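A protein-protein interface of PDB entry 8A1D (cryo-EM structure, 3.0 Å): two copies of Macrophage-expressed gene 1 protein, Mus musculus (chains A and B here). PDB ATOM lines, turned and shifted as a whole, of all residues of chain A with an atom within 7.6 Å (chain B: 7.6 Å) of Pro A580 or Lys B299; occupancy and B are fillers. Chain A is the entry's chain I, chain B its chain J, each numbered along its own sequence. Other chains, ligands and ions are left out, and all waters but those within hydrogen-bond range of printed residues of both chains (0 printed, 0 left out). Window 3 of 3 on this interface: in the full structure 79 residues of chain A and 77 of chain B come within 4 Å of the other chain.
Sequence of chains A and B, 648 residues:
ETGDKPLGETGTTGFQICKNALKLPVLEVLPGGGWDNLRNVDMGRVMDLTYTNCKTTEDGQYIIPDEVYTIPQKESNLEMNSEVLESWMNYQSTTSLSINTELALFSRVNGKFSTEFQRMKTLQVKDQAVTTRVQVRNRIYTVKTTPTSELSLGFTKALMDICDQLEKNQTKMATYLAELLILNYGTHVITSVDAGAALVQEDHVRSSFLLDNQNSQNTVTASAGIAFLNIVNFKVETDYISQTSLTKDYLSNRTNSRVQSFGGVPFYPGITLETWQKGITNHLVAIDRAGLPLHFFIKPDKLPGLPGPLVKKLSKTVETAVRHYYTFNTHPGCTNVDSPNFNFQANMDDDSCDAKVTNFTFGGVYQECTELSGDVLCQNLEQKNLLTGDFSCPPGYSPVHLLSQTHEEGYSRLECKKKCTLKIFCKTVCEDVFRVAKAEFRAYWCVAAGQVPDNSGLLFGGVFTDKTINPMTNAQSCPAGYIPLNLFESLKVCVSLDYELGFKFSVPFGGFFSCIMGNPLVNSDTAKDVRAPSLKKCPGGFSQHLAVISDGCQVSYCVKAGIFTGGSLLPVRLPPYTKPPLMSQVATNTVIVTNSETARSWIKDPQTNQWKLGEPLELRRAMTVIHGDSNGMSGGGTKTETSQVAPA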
ATOM      1  N   LYS A 172       5.131  -4.360  17.839  1.00  0.00           N
ATOM      2  CA  LYS A 172       5.310  -4.168  16.409  1.00  0.00           C
ATOM      3  C   LYS A 172       4.701  -5.316  15.620  1.00  0.00           C
ATOM      4  O   LYS A 172       3.769  -5.112  14.837  1.00  0.00           O
ATOM      5  CB  LYS A 172       6.793  -4.001  16.086  1.00  0.00           C
ATOM      6  CG  LYS A 172       7.355  -2.649  16.490  1.00  0.00           C
ATOM      7  CD  LYS A 172       6.498  -1.497  15.966  1.00  0.00           C
ATOM      8  CE  LYS A 172       6.361  -1.530  14.447  1.00  0.00           C
ATOM      9  NZ  LYS A 172       5.263  -0.652  13.959  1.00  0.00           N
ATOM     10  N   MET A 173       5.202  -6.533  15.815  1.00  0.00           N
ATOM     11  CA  MET A 173       4.593  -7.664  15.134  1.00  0.00           C
ATOM     12  C   MET A 173       3.266  -8.065  15.752  1.00  0.00           C
ATOM     13  O   MET A 173       2.543  -8.867  15.160  1.00  0.00           O
ATOM     14  CB  MET A 173       5.544  -8.859  15.102  1.00  0.00           C
ATOM     15  CG  MET A 173       6.890  -8.544  14.494  1.00  0.00           C
ATOM     16  SD  MET A 173       7.080  -9.367  12.901  1.00  0.00           S
ATOM     17  CE  MET A 173       6.922 -11.084  13.382  1.00  0.00           C
ATOM     18  N   TYR A 176       1.005  -6.260  13.374  1.00  0.00           N
ATOM     19  CA  TYR A 176       1.075  -6.973  12.105  1.00  0.00           C
ATOM     20  C   TYR A 176       0.288  -8.273  12.159  1.00  0.00           C
ATOM     21  O   TYR A 176      -0.461  -8.599  11.230  1.00  0.00           O
ATOM     22  CB  TYR A 176       2.530  -7.248  11.743  1.00  0.00           C
ATOM     23  CG  TYR A 176       2.691  -7.959  10.430  1.00  0.00           C
ATOM     24  CD1 TYR A 176       2.674  -7.262   9.235  1.00  0.00           C
ATOM     25  CD2 TYR A 176       2.866  -9.332  10.387  1.00  0.00           C
ATOM     26  CE1 TYR A 176       2.823  -7.916   8.035  1.00  0.00           C
ATOM     27  CE2 TYR A 176       3.014  -9.993   9.195  1.00  0.00           C
ATOM     28  CZ  TYR A 176       2.992  -9.280   8.020  1.00  0.00           C
ATOM     29  OH  TYR A 176       3.140  -9.937   6.822  1.00  0.00           O
ATOM     30  N   LEU A 180      -3.009  -9.408  10.056  1.00  0.00           N
ATOM     31  CA  LEU A 180      -3.128 -10.701   9.392  1.00  0.00           C
ATOM     32  C   LEU A 180      -4.405 -11.411   9.807  1.00  0.00           C
ATOM     33  O   LEU A 180      -5.069 -12.052   8.984  1.00  0.00           O
ATOM     34  CB  LEU A 180      -1.915 -11.568   9.704  1.00  0.00           C
ATOM     35  CG  LEU A 180      -0.830 -11.609   8.635  1.00  0.00           C
ATOM     36  CD1 LEU A 180      -1.075 -12.803   7.744  1.00  0.00           C
ATOM     37  CD2 LEU A 180      -0.813 -10.329   7.822  1.00  0.00           C
ATOM     38  N   PRO A 576      -1.263  -6.188   4.959  1.00  0.00           N
ATOM     39  CA  PRO A 576      -0.768  -5.262   5.977  1.00  0.00           C
ATOM     40  C   PRO A 576      -0.521  -3.877   5.415  1.00  0.00           C
ATOM     41  O   PRO A 576      -0.219  -3.712   4.237  1.00  0.00           O
ATOM     42  CB  PRO A 576       0.530  -5.929   6.425  1.00  0.00           C
ATOM     43  CG  PRO A 576       1.058  -6.532   5.156  1.00  0.00           C
ATOM     44  CD  PRO A 576      -0.164  -6.979   4.378  1.00  0.00           C
ATOM     45  N   THR A 578       1.923  -2.173   6.603  1.00  0.00           N
ATOM     46  CA  THR A 578       3.342  -2.035   6.875  1.00  0.00           C
ATOM     47  C   THR A 578       3.986  -3.402   6.704  1.00  0.00           C
ATOM     48  O   THR A 578       3.355  -4.433   6.945  1.00  0.00           O
ATOM     49  CB  THR A 578       3.605  -1.492   8.283  1.00  0.00           C
ATOM     50  OG1 THR A 578       4.989  -1.667   8.615  1.00  0.00           O
ATOM     51  CG2 THR A 578       2.746  -2.223   9.301  1.00  0.00           C
ATOM     52  N   LYS A 579       5.246  -3.395   6.277  1.00  0.00           N
ATOM     53  CA  LYS A 579       5.994  -4.631   6.161  1.00  0.00           C
ATOM     54  C   LYS A 579       6.221  -5.216   7.553  1.00  0.00           C
ATOM     55  O   LYS A 579       6.172  -4.491   8.549  1.00  0.00           O
ATOM     56  CB  LYS A 579       7.321  -4.372   5.450  1.00  0.00           C
ATOM     57  CG  LYS A 579       7.144  -3.949   4.000  1.00  0.00           C
ATOM     58  CD  LYS A 579       8.470  -3.699   3.306  1.00  0.00           C
ATOM     59  CE  LYS A 579       8.246  -3.315   1.849  1.00  0.00           C
ATOM     60  NZ  LYS A 579       9.519  -3.051   1.124  1.00  0.00           N
ATOM     61  N   PRO A 580       6.426  -6.529   7.650  1.00  0.00           N
ATOM     62  CA  PRO A 580       6.646  -7.155   8.960  1.00  0.00           C
ATOM     63  C   PRO A 580       7.761  -6.458   9.714  1.00  0.00           C
ATOM     64  O   PRO A 580       8.930  -6.504   9.304  1.00  0.00           O
ATOM     65  CB  PRO A 580       7.035  -8.596   8.602  1.00  0.00           C
ATOM     66  CG  PRO A 580       6.375  -8.837   7.307  1.00  0.00           C
ATOM     67  CD  PRO A 580       6.370  -7.528   6.568  1.00  0.00           C
ATOM     68  N   PRO A 581       7.433  -5.793  10.818  1.00  0.00           N
ATOM     69  CA  PRO A 581       8.449  -5.023  11.542  1.00  0.00           C
ATOM     70  C   PRO A 581       9.473  -5.940  12.189  1.00  0.00           C
ATOM     71  O   PRO A 581       9.146  -7.025  12.673  1.00  0.00           O
ATOM     72  CB  PRO A 581       7.631  -4.254  12.583  1.00  0.00           C
ATOM     73  CG  PRO A 581       6.410  -5.078  12.774  1.00  0.00           C
ATOM     74  CD  PRO A 581       6.111  -5.719  11.459  1.00  0.00           C
ATOM     75  N   LEU A 582      10.722  -5.490  12.194  1.00  0.00           N
ATOM     76  CA  LEU A 582      11.788  -6.272  12.795  1.00  0.00           C
ATOM     77  C   LEU A 582      11.672  -6.238  14.315  1.00  0.00           C
ATOM     78  O   LEU A 582      11.102  -5.311  14.897  1.00  0.00           O
ATOM     79  CB  LEU A 582      13.151  -5.742  12.356  1.00  0.00           C
ATOM     80  CG  LEU A 582      13.319  -5.506  10.852  1.00  0.00           C
ATOM     81  CD1 LEU A 582      14.742  -5.069  10.527  1.00  0.00           C
ATOM     82  CD2 LEU A 582      12.928  -6.734  10.045  1.00  0.00           C
ATOM     83  N   MET A 583      12.216  -7.266  14.956  1.00  0.00           N
ATOM     84  CA  MET A 583      12.180  -7.357  16.409  1.00  0.00           C
ATOM     85  C   MET A 583      13.119  -6.340  17.050  1.00  0.00           C
ATOM     86  O   MET A 583      14.261  -6.657  17.382  1.00  0.00           O
ATOM     87  CB  MET A 583      12.543  -8.771  16.864  1.00  0.00           C
ATOM     88  CG  MET A 583      11.873  -9.868  16.057  1.00  0.00           C
ATOM     89  SD  MET A 583      10.274  -9.365  15.399  1.00  0.00           S
ATOM     90  CE  MET A 583      10.387 -10.009  13.737  1.00  0.00           C
ATOM     91  N   LEU B 151       3.264 -24.354   3.580  1.00  0.00           N
ATOM     92  CA  LEU B 151       3.938 -24.376   2.296  1.00  0.00           C
ATOM     93  C   LEU B 151       4.222 -25.807   1.872  1.00  0.00           C
ATOM     94  O   LEU B 151       4.417 -26.700   2.698  1.00  0.00           O
ATOM     95  CB  LEU B 151       5.238 -23.590   2.356  1.00  0.00           C
ATOM     96  CG  LEU B 151       5.068 -22.159   2.838  1.00  0.00           C
ATOM     97  CD1 LEU B 151       6.383 -21.428   2.779  1.00  0.00           C
ATOM     98  CD2 LEU B 151       4.026 -21.444   2.019  1.00  0.00           C
ATOM     99  N   LEU B 159      13.311 -22.945  -0.732  1.00  0.00           N
ATOM    100  CA  LEU B 159      13.641 -21.859   0.180  1.00  0.00           C
ATOM    101  C   LEU B 159      14.812 -22.226   1.080  1.00  0.00           C
ATOM    102  O   LEU B 159      15.685 -21.392   1.342  1.00  0.00           O
ATOM    103  CB  LEU B 159      12.421 -21.487   1.011  1.00  0.00           C
ATOM    104  CG  LEU B 159      11.347 -20.783   0.197  1.00  0.00           C
ATOM    105  CD1 LEU B 159      10.234 -20.341   1.105  1.00  0.00           C
ATOM    106  CD2 LEU B 159      11.948 -19.606  -0.527  1.00  0.00           C
ATOM    107  N   PRO B 293       1.388 -11.401  -3.041  1.00  0.00           N
ATOM    108  CA  PRO B 293       2.789 -11.504  -3.447  1.00  0.00           C
ATOM    109  C   PRO B 293       3.483 -12.588  -2.647  1.00  0.00           C
ATOM    110  O   PRO B 293       3.197 -12.794  -1.471  1.00  0.00           O
ATOM    111  CB  PRO B 293       3.355 -10.120  -3.125  1.00  0.00           C
ATOM    112  CG  PRO B 293       2.176  -9.233  -3.114  1.00  0.00           C
ATOM    113  CD  PRO B 293       1.051 -10.049  -2.581  1.00  0.00           C
ATOM    114  N   LEU B 294       4.395 -13.302  -3.301  1.00  0.00           N
ATOM    115  CA  LEU B 294       4.925 -14.500  -2.664  1.00  0.00           C
ATOM    116  C   LEU B 294       5.898 -14.167  -1.545  1.00  0.00           C
ATOM    117  O   LEU B 294       6.164 -15.017  -0.692  1.00  0.00           O
ATOM    118  CB  LEU B 294       5.583 -15.410  -3.697  1.00  0.00           C
ATOM    119  CG  LEU B 294       7.077 -15.269  -3.921  1.00  0.00           C
ATOM    120  CD1 LEU B 294       7.558 -16.417  -4.775  1.00  0.00           C
ATOM    121  CD2 LEU B 294       7.388 -13.947  -4.577  1.00  0.00           C
ATOM    122  N   HIS B 295       6.428 -12.944  -1.511  1.00  0.00           N
ATOM    123  CA  HIS B 295       7.248 -12.569  -0.370  1.00  0.00           C
ATOM    124  C   HIS B 295       6.418 -12.450   0.893  1.00  0.00           C
ATOM    125  O   HIS B 295       6.977 -12.348   1.987  1.00  0.00           O
ATOM    126  CB  HIS B 295       7.985 -11.259  -0.633  1.00  0.00           C
ATOM    127  CG  HIS B 295       7.099 -10.058  -0.687  1.00  0.00           C
ATOM    128  ND1 HIS B 295       6.787  -9.418  -1.866  1.00  0.00           N
ATOM    129  CD2 HIS B 295       6.476  -9.364   0.294  1.00  0.00           C
ATOM    130  CE1 HIS B 295       6.003  -8.386  -1.611  1.00  0.00           C
ATOM    131  NE2 HIS B 295       5.797  -8.333  -0.307  1.00  0.00           N
ATOM    132  N   PHE B 296       5.097 -12.446   0.757  1.00  0.00           N
ATOM    133  CA  PHE B 296       4.217 -12.382   1.912  1.00  0.00           C
ATOM    134  C   PHE B 296       4.175 -13.708   2.658  1.00  0.00           C
ATOM    135  O   PHE B 296       3.877 -13.735   3.853  1.00  0.00           O
ATOM    136  CB  PHE B 296       2.822 -11.977   1.445  1.00  0.00           C
ATOM    137  CG  PHE B 296       1.805 -11.942   2.525  1.00  0.00           C
ATOM    138  CD1 PHE B 296       1.615 -10.797   3.264  1.00  0.00           C
ATOM    139  CD2 PHE B 296       1.034 -13.050   2.801  1.00  0.00           C
ATOM    140  CE1 PHE B 296       0.675 -10.757   4.258  1.00  0.00           C
ATOM    141  CE2 PHE B 296       0.096 -13.019   3.797  1.00  0.00           C
ATOM    142  CZ  PHE B 296      -0.085 -11.869   4.525  1.00  0.00           C
ATOM    143  N   PHE B 297       4.466 -14.812   1.976  1.00  0.00           N
ATOM    144  CA  PHE B 297       4.472 -16.128   2.597  1.00  0.00           C
ATOM    145  C   PHE B 297       5.816 -16.515   3.183  1.00  0.00           C
ATOM    146  O   PHE B 297       5.908 -17.556   3.840  1.00  0.00           O
ATOM    147  CB  PHE B 297       4.050 -17.191   1.589  1.00  0.00           C
ATOM    148  CG  PHE B 297       2.654 -17.033   1.108  1.00  0.00           C
ATOM    149  CD1 PHE B 297       1.604 -17.559   1.830  1.00  0.00           C
ATOM    150  CD2 PHE B 297       2.383 -16.327  -0.040  1.00  0.00           C
ATOM    151  CE1 PHE B 297       0.315 -17.411   1.399  1.00  0.00           C
ATOM    152  CE2 PHE B 297       1.095 -16.169  -0.469  1.00  0.00           C
ATOM    153  CZ  PHE B 297       0.060 -16.713   0.248  1.00  0.00           C
ATOM    154  N   ILE B 298       6.857 -15.724   2.961  1.00  0.00           N
ATOM    155  CA  ILE B 298       8.149 -16.005   3.569  1.00  0.00           C
ATOM    156  C   ILE B 298       8.201 -15.298   4.913  1.00  0.00           C
ATOM    157  O   ILE B 298       8.674 -14.162   5.017  1.00  0.00           O
ATOM    158  CB  ILE B 298       9.296 -15.573   2.645  1.00  0.00           C
ATOM    159  CG1 ILE B 298       9.110 -16.213   1.273  1.00  0.00           C
ATOM    160  CG2 ILE B 298      10.628 -15.967   3.232  1.00  0.00           C
ATOM    161  CD1 ILE B 298      10.181 -15.863   0.294  1.00  0.00           C
ATOM    162  N   LYS B 299       7.700 -15.960   5.945  1.00  0.00           N
ATOM    163  CA  LYS B 299       7.584 -15.386   7.274  1.00  0.00           C
ATOM    164  C   LYS B 299       8.123 -16.385   8.281  1.00  0.00           C
ATOM    165  O   LYS B 299       8.065 -17.598   8.052  1.00  0.00           O
ATOM    166  CB  LYS B 299       6.128 -15.039   7.605  1.00  0.00           C
ATOM    167  CG  LYS B 299       5.532 -13.998   6.689  1.00  0.00           C
ATOM    168  CD  LYS B 299       6.293 -12.698   6.771  1.00  0.00           C
ATOM    169  CE  LYS B 299       6.011 -11.847   5.555  1.00  0.00           C
ATOM    170  NZ  LYS B 299       6.548 -12.486   4.326  1.00  0.00           N
ATOM    171  N   PRO B 300       8.653 -15.908   9.410  1.00  0.00           N
ATOM    172  CA  PRO B 300       9.255 -16.838  10.376  1.00  0.00           C
ATOM    173  C   PRO B 300       8.301 -17.914  10.848  1.00  0.00           C
ATOM    174  O   PRO B 300       8.694 -19.081  10.967  1.00  0.00           O
ATOM    175  CB  PRO B 300       9.675 -15.916  11.527  1.00  0.00           C
ATOM    176  CG  PRO B 300       9.801 -14.570  10.913  1.00  0.00           C
ATOM    177  CD  PRO B 300       8.769 -14.506   9.840  1.00  0.00           C
ATOM    178  N   ASP B 301       7.045 -17.559  11.089  1.00  0.00           N
ATOM    179  CA  ASP B 301       6.054 -18.518  11.553  1.00  0.00           C
ATOM    180  C   ASP B 301       5.690 -19.539  10.493  1.00  0.00           C
ATOM    181  O   ASP B 301       5.057 -20.549  10.815  1.00  0.00           O
ATOM    182  CB  ASP B 301       4.790 -17.785  11.999  1.00  0.00           C
ATOM    183  CG  ASP B 301       4.197 -16.938  10.893  1.00  0.00           C
ATOM    184  OD1 ASP B 301       4.832 -16.832   9.825  1.00  0.00           O
ATOM    185  OD2 ASP B 301       3.096 -16.384  11.088  1.00  0.00           O
ATOM    186  N   LYS B 302       6.068 -19.294   9.244  1.00  0.00           N
ATOM    187  CA  LYS B 302       5.717 -20.167   8.138  1.00  0.00           C
ATOM    188  C   LYS B 302       6.804 -21.171   7.802  1.00  0.00           C
ATOM    189  O   LYS B 302       6.509 -22.206   7.205  1.00  0.00           O
ATOM    190  CB  LYS B 302       5.404 -19.329   6.895  1.00  0.00           C
ATOM    191  CG  LYS B 302       4.695 -20.086   5.803  1.00  0.00           C
ATOM    192  CD  LYS B 302       3.330 -20.553   6.263  1.00  0.00           C
ATOM    193  CE  LYS B 302       2.416 -19.378   6.544  1.00  0.00           C
ATOM    194  NZ  LYS B 302       1.068 -19.841   6.957  1.00  0.00           N
ATOM    195  N   LEU B 303       8.051 -20.893   8.182  1.00  0.00           N
ATOM    196  CA  LEU B 303       9.178 -21.791   7.949  1.00  0.00           C
ATOM    197  C   LEU B 303       9.778 -22.198   9.285  1.00  0.00           C
ATOM    198  O   LEU B 303      10.590 -21.460   9.861  1.00  0.00           O
ATOM    199  CB  LEU B 303      10.226 -21.122   7.062  1.00  0.00           C
ATOM    200  CG  LEU B 303       9.666 -20.723   5.706  1.00  0.00           C
ATOM    201  CD1 LEU B 303      10.696 -19.990   4.887  1.00  0.00           C
ATOM    202  CD2 LEU B 303       9.218 -21.968   4.990  1.00  0.00           C
ATOM    203  N   PRO B 304       9.398 -23.353   9.832  1.00  0.00           N
ATOM    204  CA  PRO B 304       9.995 -23.788  11.101  1.00  0.00           C
ATOM    205  C   PRO B 304      11.492 -24.018  11.017  1.00  0.00           C
ATOM    206  O   PRO B 304      12.201 -23.760  11.996  1.00  0.00           O
ATOM    207  CB  PRO B 304       9.246 -25.092  11.413  1.00  0.00           C
ATOM    208  CG  PRO B 304       8.026 -25.066  10.544  1.00  0.00           C
ATOM    209  CD  PRO B 304       8.422 -24.323   9.316  1.00  0.00           C
ATOM    210  N   LEU B 306      13.906 -22.526   9.718  1.00  0.00           N
ATOM    211  CA  LEU B 306      14.960 -21.519   9.729  1.00  0.00           C
ATOM    212  C   LEU B 306      14.710 -20.479  10.822  1.00  0.00           C
ATOM    213  O   LEU B 306      13.568 -20.289  11.249  1.00  0.00           O
ATOM    214  CB  LEU B 306      15.047 -20.836   8.371  1.00  0.00           C
ATOM    215  CG  LEU B 306      15.152 -21.844   7.225  1.00  0.00           C
ATOM    216  CD1 LEU B 306      15.086 -21.159   5.880  1.00  0.00           C
ATOM    217  CD2 LEU B 306      16.432 -22.654   7.354  1.00  0.00           C
ATOM    218  N   PRO B 307      15.759 -19.819  11.303  1.00  0.00           N
ATOM    219  CA  PRO B 307      15.577 -18.745  12.285  1.00  0.00           C
ATOM    220  C   PRO B 307      15.020 -17.488  11.636  1.00  0.00           C
ATOM    221  O   PRO B 307      15.081 -17.291  10.422  1.00  0.00           O
ATOM    222  CB  PRO B 307      16.990 -18.506  12.828  1.00  0.00           C
ATOM    223  CG  PRO B 307      17.786 -19.700  12.397  1.00  0.00           C
ATOM    224  CD  PRO B 307      17.180 -20.145  11.110  1.00  0.00           C
ATOM    225  N   GLY B 308      14.480 -16.616  12.482  1.00  0.00           N
ATOM    226  CA  GLY B 308      13.856 -15.391  12.036  1.00  0.00           C
ATOM    227  C   GLY B 308      14.761 -14.432  11.282  1.00  0.00           C
ATOM    228  O   GLY B 308      14.413 -13.945  10.199  1.00  0.00           O
ATOM    229  N   VAL B 311      15.251 -15.731   7.763  1.00  0.00           N
ATOM    230  CA  VAL B 311      14.120 -15.642   6.851  1.00  0.00           C
ATOM    231  C   VAL B 311      13.855 -14.194   6.480  1.00  0.00           C
ATOM    232  O   VAL B 311      13.288 -13.917   5.421  1.00  0.00           O
ATOM    233  CB  VAL B 311      12.869 -16.309   7.445  1.00  0.00           C
ATOM    234  CG1 VAL B 311      13.162 -17.752   7.805  1.00  0.00           C
ATOM    235  CG2 VAL B 311      12.360 -15.542   8.632  1.00  0.00           C
ATOM    236  N   LYS B 312      14.260 -13.247   7.325  1.00  0.00           N
ATOM    237  CA  LYS B 312      14.151 -11.845   6.935  1.00  0.00           C
ATOM    238  C   LYS B 312      14.990 -11.562   5.696  1.00  0.00           C
ATOM    239  O   LYS B 312      14.507 -10.971   4.721  1.00  0.00           O
ATOM    240  CB  LYS B 312      14.580 -10.953   8.094  1.00  0.00           C
ATOM    241  CG  LYS B 312      13.589 -10.939   9.229  1.00  0.00           C
ATOM    242  CD  LYS B 312      14.083 -10.083  10.371  1.00  0.00           C
ATOM    243  CE  LYS B 312      13.092 -10.098  11.514  1.00  0.00           C
ATOM    244  NZ  LYS B 312      12.873 -11.474  12.036  1.00  0.00           N
ATOM    245  N   SER B 315      13.405 -13.236   2.655  1.00  0.00           N
ATOM    246  CA  SER B 315      12.331 -12.450   2.071  1.00  0.00           C
ATOM    247  C   SER B 315      12.889 -11.263   1.311  1.00  0.00           C
ATOM    248  O   SER B 315      12.407 -10.934   0.223  1.00  0.00           O
ATOM    249  CB  SER B 315      11.367 -11.988   3.158  1.00  0.00           C
ATOM    250  OG  SER B 315      10.319 -11.217   2.601  1.00  0.00           O
ATOM    251  N   GLU B 319      12.274 -10.828  -2.644  1.00  0.00           N
ATOM    252  CA  GLU B 319      11.575  -9.643  -3.115  1.00  0.00           C
ATOM    253  C   GLU B 319      12.416  -8.876  -4.122  1.00  0.00           C
ATOM    254  O   GLU B 319      11.889  -8.371  -5.117  1.00  0.00           O
ATOM    255  CB  GLU B 319      11.194  -8.760  -1.932  1.00  0.00           C
ATOM    256  CG  GLU B 319      10.332  -7.576  -2.308  1.00  0.00           C
ATOM    257  CD  GLU B 319       9.821  -6.827  -1.098  1.00  0.00           C
ATOM    258  OE1 GLU B 319      10.150  -7.237   0.035  1.00  0.00           O
ATOM    259  OE2 GLU B 319       9.083  -5.835  -1.277  1.00  0.00           O
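The side-chain amino group of Lys A579 lies within salt-bridge range of the side-chain carboxylate of Glu B319, 3.7 Å away.
The side-chain amino group of Lys B299 lies within hydrogen-bond range of the backbone carbonyl oxygen of Phe B296.
The backbone carbonyl oxygen of Gly B308 sits close to the side-chain amino group of Lys B312, at 3.4 Å.
Among the printed residues, merely in contact across the chains: Met A583 with Lys B312, Leu A180 with Phe B296, Pro A580 with Lys B299, Leu A582 with Lys B312, Tyr A176 with Phe B296, Tyr A176 with Lys B299 and Pro A576 with Phe B296.
Printed residues of chain B within 4 Å of Leu A180: Phe B296.
Of the printed residues of chain B, Pro A576 touches Phe B296 (3.9 Å).
Of the printed residues of chain B, Lys A579 touches Glu B319 (3.7 Å).
Pro A580 touches one residue of chain B.
Of the printed residues of chain A, Phe B296 touches Tyr A176 (3.7 Å), Leu A180 (3.5 Å) and Pro A576 (3.9 Å).
Lys B299 touches two residues of chain A.
Gly B308 touches none of the printed residues of chain A.
Val B311 touches none of the printed residues of chain A.
Of the printed residues of chain A, Glu B319 touches Lys A579 (3.7 Å).
The nearest residue of chain B that does not touch Pro A580 is Lys B312 (5.9 Å).
The nearest printed residue of chain A that does not touch Glu B319 is Pro A580 (7.6 Å).
Of the 11 printed residues of chain A, 7 touch a printed residue of chain B.
Hydrophobic or aromatic side chains of chain A that line the printed part of chain B: Tyr A176, Leu A180, Pro A576, Pro A580, Leu A582 and Met A583.
Among the printed residues, Asp or Glu carboxylates within 4 Å of a Lys or Arg side-chain nitrogen of the other chain: Lys A579 with Glu B319.
No position is printed for both chains.
Of the 8 pairs that touch across the chains among the printed residues, none has its exchanged pair printed and touching as well.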
